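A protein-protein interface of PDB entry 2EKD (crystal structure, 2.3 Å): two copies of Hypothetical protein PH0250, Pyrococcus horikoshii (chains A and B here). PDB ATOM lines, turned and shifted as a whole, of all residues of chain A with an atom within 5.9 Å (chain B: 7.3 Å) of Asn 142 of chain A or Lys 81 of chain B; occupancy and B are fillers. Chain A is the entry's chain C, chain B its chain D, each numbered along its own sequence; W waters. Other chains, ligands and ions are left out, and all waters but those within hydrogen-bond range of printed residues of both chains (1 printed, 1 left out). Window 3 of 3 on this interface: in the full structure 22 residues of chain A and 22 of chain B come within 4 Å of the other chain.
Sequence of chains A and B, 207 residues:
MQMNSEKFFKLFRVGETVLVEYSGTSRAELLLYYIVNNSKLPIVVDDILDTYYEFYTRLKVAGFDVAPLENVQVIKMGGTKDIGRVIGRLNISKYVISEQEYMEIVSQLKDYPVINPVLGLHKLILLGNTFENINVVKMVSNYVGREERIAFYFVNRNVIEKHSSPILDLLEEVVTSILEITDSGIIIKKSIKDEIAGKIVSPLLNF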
ATOM      1  N   GLU A  99      17.696 -12.105 -36.864  1.00  0.00           N
ATOM      2  CA  GLU A  99      19.029 -11.538 -36.699  1.00  0.00           C
ATOM      3  C   GLU A  99      19.642 -11.194 -38.057  1.00  0.00           C
ATOM      4  O   GLU A  99      20.560 -10.387 -38.180  1.00  0.00           O
ATOM      5  CB  GLU A  99      19.918 -12.559 -35.964  1.00  0.00           C
ATOM      6  CG  GLU A  99      21.373 -12.085 -35.816  1.00  0.00           C
ATOM      7  CD  GLU A  99      22.202 -13.125 -35.082  1.00  0.00           C
ATOM      8  OE1 GLU A  99      22.346 -14.229 -35.584  1.00  0.00           O
ATOM      9  OE2 GLU A  99      22.743 -12.806 -34.028  1.00  0.00           O
ATOM     10  N   VAL A 137      15.926 -13.543 -25.009  1.00  0.00           N
ATOM     11  CA  VAL A 137      17.141 -13.395 -24.213  1.00  0.00           C
ATOM     12  C   VAL A 137      18.371 -13.749 -25.057  1.00  0.00           C
ATOM     13  O   VAL A 137      19.408 -13.092 -24.965  1.00  0.00           O
ATOM     14  CB  VAL A 137      17.113 -14.292 -22.958  1.00  0.00           C
ATOM     15  CG1 VAL A 137      18.468 -14.235 -22.241  1.00  0.00           C
ATOM     16  CG2 VAL A 137      15.999 -13.832 -22.023  1.00  0.00           C
ATOM     17  N   LYS A 138      18.253 -14.786 -25.878  1.00  0.00           N
ATOM     18  CA  LYS A 138      19.359 -15.192 -26.736  1.00  0.00           C
ATOM     19  C   LYS A 138      19.682 -14.062 -27.702  1.00  0.00           C
ATOM     20  O   LYS A 138      20.843 -13.837 -28.040  1.00  0.00           O
ATOM     21  CB  LYS A 138      19.004 -16.461 -27.519  1.00  0.00           C
ATOM     22  CG  LYS A 138      20.030 -16.829 -28.582  1.00  0.00           C
ATOM     23  CD  LYS A 138      20.414 -18.304 -28.533  1.00  0.00           C
ATOM     24  CE  LYS A 138      21.223 -18.633 -27.280  1.00  0.00           C
ATOM     25  NZ  LYS A 138      21.678 -20.055 -27.271  1.00  0.00           N
ATOM     26  N   MET A 139      18.649 -13.354 -28.147  1.00  0.00           N
ATOM     27  CA  MET A 139      18.836 -12.236 -29.064  1.00  0.00           C
ATOM     28  C   MET A 139      19.740 -11.211 -28.389  1.00  0.00           C
ATOM     29  O   MET A 139      20.705 -10.735 -28.977  1.00  0.00           O
ATOM     30  CB  MET A 139      17.490 -11.586 -29.394  1.00  0.00           C
ATOM     31  CG  MET A 139      17.555 -10.517 -30.472  1.00  0.00           C
ATOM     32  SD  MET A 139      16.077  -9.462 -30.512  1.00  0.00           S
ATOM     33  CE  MET A 139      14.762 -10.693 -30.632  1.00  0.00           C
ATOM     34  N   VAL A 140      19.425 -10.887 -27.139  1.00  0.00           N
ATOM     35  CA  VAL A 140      20.199  -9.919 -26.371  1.00  0.00           C
ATOM     36  C   VAL A 140      21.640 -10.374 -26.140  1.00  0.00           C
ATOM     37  O   VAL A 140      22.575  -9.580 -26.277  1.00  0.00           O
ATOM     38  CB  VAL A 140      19.537  -9.641 -24.998  1.00  0.00           C
ATOM     39  CG1 VAL A 140      20.369  -8.624 -24.214  1.00  0.00           C
ATOM     40  CG2 VAL A 140      18.107  -9.132 -25.203  1.00  0.00           C
ATOM     41  N   SER A 141      21.832 -11.648 -25.804  1.00  0.00           N
ATOM     42  CA  SER A 141      23.186 -12.135 -25.563  1.00  0.00           C
ATOM     43  C   SER A 141      24.025 -12.236 -26.844  1.00  0.00           C
ATOM     44  O   SER A 141      25.254 -12.175 -26.786  1.00  0.00           O
ATOM     45  CB  SER A 141      23.159 -13.484 -24.830  1.00  0.00           C
ATOM     46  OG  SER A 141      22.588 -14.518 -25.610  1.00  0.00           O
ATOM     47  N   ASN A 142      23.372 -12.364 -27.996  1.00  0.00           N
ATOM     48  CA  ASN A 142      24.108 -12.463 -29.252  1.00  0.00           C
ATOM     49  C   ASN A 142      24.824 -11.178 -29.648  1.00  0.00           C
ATOM     50  O   ASN A 142      25.744 -11.211 -30.458  1.00  0.00           O
ATOM     51  CB  ASN A 142      23.186 -12.867 -30.404  1.00  0.00           C
ATOM     52  CG  ASN A 142      22.954 -14.359 -30.466  1.00  0.00           C
ATOM     53  OD1 ASN A 142      23.762 -15.147 -29.963  1.00  0.00           O
ATOM     54  ND2 ASN A 142      21.857 -14.761 -31.101  1.00  0.00           N
ATOM     55  N   TYR A 143      24.402 -10.052 -29.084  1.00  0.00           N
ATOM     56  CA  TYR A 143      25.011  -8.770 -29.422  1.00  0.00           C
ATOM     57  C   TYR A 143      25.930  -8.208 -28.351  1.00  0.00           C
ATOM     58  O   TYR A 143      26.603  -7.199 -28.573  1.00  0.00           O
ATOM     59  CB  TYR A 143      23.917  -7.755 -29.763  1.00  0.00           C
ATOM     60  CG  TYR A 143      23.106  -8.182 -30.961  1.00  0.00           C
ATOM     61  CD1 TYR A 143      23.704  -8.311 -32.214  1.00  0.00           C
ATOM     62  CD2 TYR A 143      21.757  -8.501 -30.838  1.00  0.00           C
ATOM     63  CE1 TYR A 143      22.978  -8.749 -33.314  1.00  0.00           C
ATOM     64  CE2 TYR A 143      21.021  -8.942 -31.930  1.00  0.00           C
ATOM     65  CZ  TYR A 143      21.638  -9.062 -33.165  1.00  0.00           C
ATOM     66  OH  TYR A 143      20.915  -9.487 -34.250  1.00  0.00           O
ATOM     67  N   VAL A 144      25.956  -8.854 -27.189  1.00  0.00           N
ATOM     68  CA  VAL A 144      26.824  -8.411 -26.107  1.00  0.00           C
ATOM     69  C   VAL A 144      28.261  -8.406 -26.616  1.00  0.00           C
ATOM     70  O   VAL A 144      28.730  -9.392 -27.183  1.00  0.00           O
ATOM     71  CB  VAL A 144      26.737  -9.352 -24.876  1.00  0.00           C
ATOM     72  CG1 VAL A 144      27.808  -8.982 -23.850  1.00  0.00           C
ATOM     73  CG2 VAL A 144      25.368  -9.246 -24.239  1.00  0.00           C
ATOM     74  N   ASP B  47      29.703 -27.396 -22.450  1.00  0.00           N
ATOM     75  CA  ASP B  47      28.992 -26.185 -22.858  1.00  0.00           C
ATOM     76  C   ASP B  47      27.572 -26.446 -23.360  1.00  0.00           C
ATOM     77  O   ASP B  47      27.370 -26.859 -24.495  1.00  0.00           O
ATOM     78  CB  ASP B  47      29.838 -25.481 -23.931  1.00  0.00           C
ATOM     79  CG  ASP B  47      29.154 -24.279 -24.541  1.00  0.00           C
ATOM     80  OD1 ASP B  47      28.196 -23.741 -23.944  1.00  0.00           O
ATOM     81  OD2 ASP B  47      29.597 -23.858 -25.628  1.00  0.00           O
ATOM     82  N   LEU B  49      23.975 -25.352 -24.671  1.00  0.00           N
ATOM     83  CA  LEU B  49      23.278 -24.294 -25.386  1.00  0.00           C
ATOM     84  C   LEU B  49      24.019 -22.965 -25.458  1.00  0.00           C
ATOM     85  O   LEU B  49      23.470 -21.912 -25.135  1.00  0.00           O
ATOM     86  CB  LEU B  49      21.882 -24.100 -24.787  1.00  0.00           C
ATOM     87  CG  LEU B  49      20.964 -25.309 -25.010  1.00  0.00           C
ATOM     88  CD1 LEU B  49      19.754 -25.239 -24.080  1.00  0.00           C
ATOM     89  CD2 LEU B  49      20.534 -25.358 -26.479  1.00  0.00           C
ATOM     90  N   ASP B  50      25.272 -23.036 -25.895  1.00  0.00           N
ATOM     91  CA  ASP B  50      26.134 -21.871 -26.064  1.00  0.00           C
ATOM     92  C   ASP B  50      26.283 -20.962 -24.855  1.00  0.00           C
ATOM     93  O   ASP B  50      26.421 -19.747 -25.001  1.00  0.00           O
ATOM     94  CB  ASP B  50      25.660 -21.044 -27.258  1.00  0.00           C
ATOM     95  CG  ASP B  50      25.753 -21.803 -28.561  1.00  0.00           C
ATOM     96  OD1 ASP B  50      26.701 -22.603 -28.712  1.00  0.00           O
ATOM     97  OD2 ASP B  50      24.887 -21.589 -29.435  1.00  0.00           O
ATOM     98  N   THR B  51      26.270 -21.546 -23.664  1.00  0.00           N
ATOM     99  CA  THR B  51      26.422 -20.765 -22.446  1.00  0.00           C
ATOM    100  C   THR B  51      27.882 -20.360 -22.243  1.00  0.00           C
ATOM    101  O   THR B  51      28.169 -19.321 -21.648  1.00  0.00           O
ATOM    102  CB  THR B  51      25.915 -21.564 -21.235  1.00  0.00           C
ATOM    103  OG1 THR B  51      24.530 -21.878 -21.439  1.00  0.00           O
ATOM    104  CG2 THR B  51      26.067 -20.758 -19.941  1.00  0.00           C
ATOM    105  N   TYR B  52      28.804 -21.176 -22.749  1.00  0.00           N
ATOM    106  CA  TYR B  52      30.229 -20.885 -22.619  1.00  0.00           C
ATOM    107  C   TYR B  52      30.575 -19.610 -23.391  1.00  0.00           C
ATOM    108  O   TYR B  52      31.420 -18.825 -22.974  1.00  0.00           O
ATOM    109  CB  TYR B  52      31.058 -22.062 -23.137  1.00  0.00           C
ATOM    110  CG  TYR B  52      32.536 -21.990 -22.787  1.00  0.00           C
ATOM    111  CD1 TYR B  52      32.963 -21.432 -21.582  1.00  0.00           C
ATOM    112  CD2 TYR B  52      33.504 -22.513 -23.647  1.00  0.00           C
ATOM    113  CE1 TYR B  52      34.316 -21.396 -21.238  1.00  0.00           C
ATOM    114  CE2 TYR B  52      34.866 -22.484 -23.311  1.00  0.00           C
ATOM    115  CZ  TYR B  52      35.259 -21.926 -22.106  1.00  0.00           C
ATOM    116  OH  TYR B  52      36.589 -21.918 -21.758  1.00  0.00           O
ATOM    117  N   TYR B  53      29.909 -19.409 -24.518  1.00  0.00           N
ATOM    118  CA  TYR B  53      30.129 -18.232 -25.342  1.00  0.00           C
ATOM    119  C   TYR B  53      29.668 -16.964 -24.606  1.00  0.00           C
ATOM    120  O   TYR B  53      30.262 -15.893 -24.765  1.00  0.00           O
ATOM    121  CB  TYR B  53      29.358 -18.380 -26.655  1.00  0.00           C
ATOM    122  CG  TYR B  53      29.242 -17.108 -27.470  1.00  0.00           C
ATOM    123  CD1 TYR B  53      30.257 -16.714 -28.340  1.00  0.00           C
ATOM    124  CD2 TYR B  53      28.112 -16.286 -27.361  1.00  0.00           C
ATOM    125  CE1 TYR B  53      30.155 -15.535 -29.083  1.00  0.00           C
ATOM    126  CE2 TYR B  53      28.002 -15.101 -28.097  1.00  0.00           C
ATOM    127  CZ  TYR B  53      29.026 -14.734 -28.954  1.00  0.00           C
ATOM    128  OH  TYR B  53      28.937 -13.555 -29.663  1.00  0.00           O
ATOM    129  N   GLU B  54      28.607 -17.086 -23.811  1.00  0.00           N
ATOM    130  CA  GLU B  54      28.072 -15.942 -23.067  1.00  0.00           C
ATOM    131  C   GLU B  54      29.056 -15.506 -21.988  1.00  0.00           C
ATOM    132  O   GLU B  54      29.311 -14.313 -21.820  1.00  0.00           O
ATOM    133  CB  GLU B  54      26.710 -16.297 -22.452  1.00  0.00           C
ATOM    134  CG  GLU B  54      25.739 -16.899 -23.473  1.00  0.00           C
ATOM    135  CD  GLU B  54      24.353 -17.185 -22.915  1.00  0.00           C
ATOM    136  OE1 GLU B  54      24.246 -17.715 -21.787  1.00  0.00           O
ATOM    137  OE2 GLU B  54      23.364 -16.891 -23.622  1.00  0.00           O
ATOM    138  N   THR B  57      32.156 -14.036 -23.699  1.00  0.00           N
ATOM    139  CA  THR B  57      31.839 -12.707 -24.207  1.00  0.00           C
ATOM    140  C   THR B  57      31.810 -11.634 -23.112  1.00  0.00           C
ATOM    141  O   THR B  57      32.288 -10.516 -23.318  1.00  0.00           O
ATOM    142  CB  THR B  57      30.473 -12.732 -24.954  1.00  0.00           C
ATOM    143  OG1 THR B  57      30.633 -13.411 -26.209  1.00  0.00           O
ATOM    144  CG2 THR B  57      29.972 -11.340 -25.217  1.00  0.00           C
ATOM    145  N   VAL B  74      36.522 -28.597 -25.023  1.00  0.00           N
ATOM    146  CA  VAL B  74      35.104 -28.379 -24.797  1.00  0.00           C
ATOM    147  C   VAL B  74      34.186 -29.409 -25.441  1.00  0.00           C
ATOM    148  O   VAL B  74      34.422 -29.854 -26.566  1.00  0.00           O
ATOM    149  CB  VAL B  74      34.690 -26.977 -25.317  1.00  0.00           C
ATOM    150  CG1 VAL B  74      33.200 -26.751 -25.113  1.00  0.00           C
ATOM    151  CG2 VAL B  74      35.487 -25.905 -24.600  1.00  0.00           C
ATOM    152  N   LYS B  76      30.418 -29.631 -26.555  1.00  0.00           N
ATOM    153  CA  LYS B  76      29.196 -28.874 -26.753  1.00  0.00           C
ATOM    154  C   LYS B  76      27.963 -29.759 -26.733  1.00  0.00           C
ATOM    155  O   LYS B  76      27.969 -30.882 -27.243  1.00  0.00           O
ATOM    156  CB  LYS B  76      29.228 -28.109 -28.077  1.00  0.00           C
ATOM    157  CG  LYS B  76      30.215 -26.964 -28.120  1.00  0.00           C
ATOM    158  CD  LYS B  76      30.068 -26.180 -29.425  1.00  0.00           C
ATOM    159  CE  LYS B  76      28.790 -25.358 -29.453  1.00  0.00           C
ATOM    160  NZ  LYS B  76      28.811 -24.275 -28.419  1.00  0.00           N
ATOM    161  N   GLY B  78      24.353 -29.090 -27.905  1.00  0.00           N
ATOM    162  CA  GLY B  78      23.486 -28.161 -28.605  1.00  0.00           C
ATOM    163  C   GLY B  78      24.331 -26.936 -28.906  1.00  0.00           C
ATOM    164  O   GLY B  78      25.549 -26.988 -28.755  1.00  0.00           O
ATOM    165  N   GLY B  79      23.707 -25.841 -29.335  1.00  0.00           N
ATOM    166  CA  GLY B  79      24.460 -24.626 -29.605  1.00  0.00           C
ATOM    167  C   GLY B  79      25.167 -24.533 -30.946  1.00  0.00           C
ATOM    168  O   GLY B  79      25.441 -25.545 -31.583  1.00  0.00           O
ATOM    169  N   THR B  80      25.472 -23.306 -31.365  1.00  0.00           N
ATOM    170  CA  THR B  80      26.139 -23.056 -32.640  1.00  0.00           C
ATOM    171  C   THR B  80      27.357 -22.134 -32.515  1.00  0.00           C
ATOM    172  O   THR B  80      28.020 -21.843 -33.516  1.00  0.00           O
ATOM    173  CB  THR B  80      25.177 -22.403 -33.648  1.00  0.00           C
ATOM    174  OG1 THR B  80      24.726 -21.148 -33.123  1.00  0.00           O
ATOM    175  CG2 THR B  80      23.972 -23.307 -33.912  1.00  0.00           C
ATOM    176  N   LYS B  81      27.640 -21.671 -31.298  1.00  0.00           N
ATOM    177  CA  LYS B  81      28.771 -20.777 -31.046  1.00  0.00           C
ATOM    178  C   LYS B  81      29.951 -21.571 -30.483  1.00  0.00           C
ATOM    179  O   LYS B  81      29.915 -22.030 -29.337  1.00  0.00           O
ATOM    180  CB  LYS B  81      28.378 -19.693 -30.039  1.00  0.00           C
ATOM    181  CG  LYS B  81      27.196 -18.824 -30.427  1.00  0.00           C
ATOM    182  CD  LYS B  81      27.536 -17.881 -31.561  1.00  0.00           C
ATOM    183  CE  LYS B  81      26.546 -16.723 -31.626  1.00  0.00           C
ATOM    184  NZ  LYS B  81      25.135 -17.181 -31.791  1.00  0.00           N
ATOM    185  N   ASP B  82      31.000 -21.725 -31.282  1.00  0.00           N
ATOM    186  CA  ASP B  82      32.173 -22.472 -30.848  1.00  0.00           C
ATOM    187  C   ASP B  82      33.207 -21.629 -30.110  1.00  0.00           C
ATOM    188  O   ASP B  82      33.678 -20.612 -30.618  1.00  0.00           O
ATOM    189  CB  ASP B  82      32.841 -23.135 -32.051  1.00  0.00           C
ATOM    190  CG  ASP B  82      32.031 -24.286 -32.606  1.00  0.00           C
ATOM    191  OD1 ASP B  82      30.834 -24.399 -32.263  1.00  0.00           O
ATOM    192  OD2 ASP B  82      32.595 -25.073 -33.395  1.00  0.00           O
ATOM    193  N   ILE B  83      33.550 -22.063 -28.902  1.00  0.00           N
ATOM    194  CA  ILE B  83      34.556 -21.395 -28.090  1.00  0.00           C
ATOM    195  C   ILE B  83      35.434 -22.485 -27.485  1.00  0.00           C
ATOM    196  O   ILE B  83      34.927 -23.416 -26.857  1.00  0.00           O
ATOM    197  CB  ILE B  83      33.931 -20.584 -26.941  1.00  0.00           C
ATOM    198  CG1 ILE B  83      33.072 -19.451 -27.500  1.00  0.00           C
ATOM    199  CG2 ILE B  83      35.035 -20.022 -26.050  1.00  0.00           C
ATOM    200  CD1 ILE B  83      33.837 -18.455 -28.352  1.00  0.00           C
ATOM    201  N   GLY B  84      36.744 -22.369 -27.678  1.00  0.00           N
ATOM    202  CA  GLY B  84      37.663 -23.359 -27.141  1.00  0.00           C
ATOM    203  C   GLY B  84      37.898 -24.510 -28.107  1.00  0.00           C
ATOM    204  O   GLY B  84      37.409 -24.490 -29.240  1.00  0.00           O
ATOM    205  N   VAL B  86      36.839 -27.618 -29.274  1.00  0.00           N
ATOM    206  CA  VAL B  86      35.686 -28.509 -29.250  1.00  0.00           C
ATOM    207  C   VAL B  86      36.061 -29.937 -29.628  1.00  0.00           C
ATOM    208  O   VAL B  86      36.357 -30.220 -30.790  1.00  0.00           O
ATOM    209  CB  VAL B  86      34.588 -28.014 -30.223  1.00  0.00           C
ATOM    210  CG1 VAL B  86      33.433 -28.996 -30.256  1.00  0.00           C
ATOM    211  CG2 VAL B  86      34.096 -26.639 -29.792  1.00  0.00           C
HETATM  212  O   HOH W   1      24.046 -18.052 -26.216  1.00  0.00           O
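Water W1 lies within hydrogen-bond range of OE2 of Glu 54 of chain B (2.9 Å), O of Asp 50 of chain B (3.2 Å) and NZ of Lys 138 of chain A (3.3 Å).
O of Lys 138 of chain A lies within hydrogen-bond range of OG of Ser 141 of chain A (3.1 Å).
The side-chain amide nitrogen of Asn 142 of chain A lies close to the backbone carbonyl oxygen of Lys 138 of chain A (3.4 Å).
N of Lys 81 of chain B sits at hydrogen-bond distance from OD1 of Asp 50 of chain B, at 2.9 Å.
O of Tyr 53 of chain B lies within hydrogen-bond range of OG1 of Thr 57 of chain B, at 2.9 Å.
NZ of Lys 76 of chain B sits at hydrogen-bond distance from O of Lys 81 of chain B.
Printed residues of chain B within 4 Å of Lys 138 of chain A: Leu 49.
Of the printed residues of chain B, Val 144 of chain A touches Thr 57 (3.0 Å).
Printed residues of chain A within 4 Å of Leu 49 of chain B: Lys 138.
The nearest printed residue of chain B that does not touch Val 144 of chain A is Tyr 53 of chain B (4.9 Å).
Thr 57 of chain B touches Val 144 of chain A (CG2 to O, 3.0 Å).
O of Leu 49 of chain B lies within hydrogen-bond range of NZ of Lys 138 of chain A, at 3.3 Å.
OG of Ser 141 of chain A lies within hydrogen-bond range of OE2 of Glu 54 of chain B (3.2 Å).
NZ of Lys 81 of chain B lies within hydrogen-bond range of OD1 of Asn 142 of chain A.
Of the 9 printed residues of chain A, 4 touch a printed residue of chain B.
Printed residues of chain A that touch a printed residue of chain B: Lys 138, Ser 141, Asn 142 and Val 144.
Hydrophobic or aromatic side chains of chain A within 4 Å of the printed part of chain B: Val 144.
Of the 18 printed residues of chain B, 4 touch a printed residue of chain A.
Along chain B the printed residues that touch a printed residue of chain A span positions 49 to 81.
Among the printed residues, no Asp or Glu carboxylate lies within 4 Å of a Lys or Arg side-chain nitrogen of the other chain.
No position is printed for both chains.
Of the 4 pairs that touch across the chains among the printed residues, none has its exchanged pair printed and touching as well.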
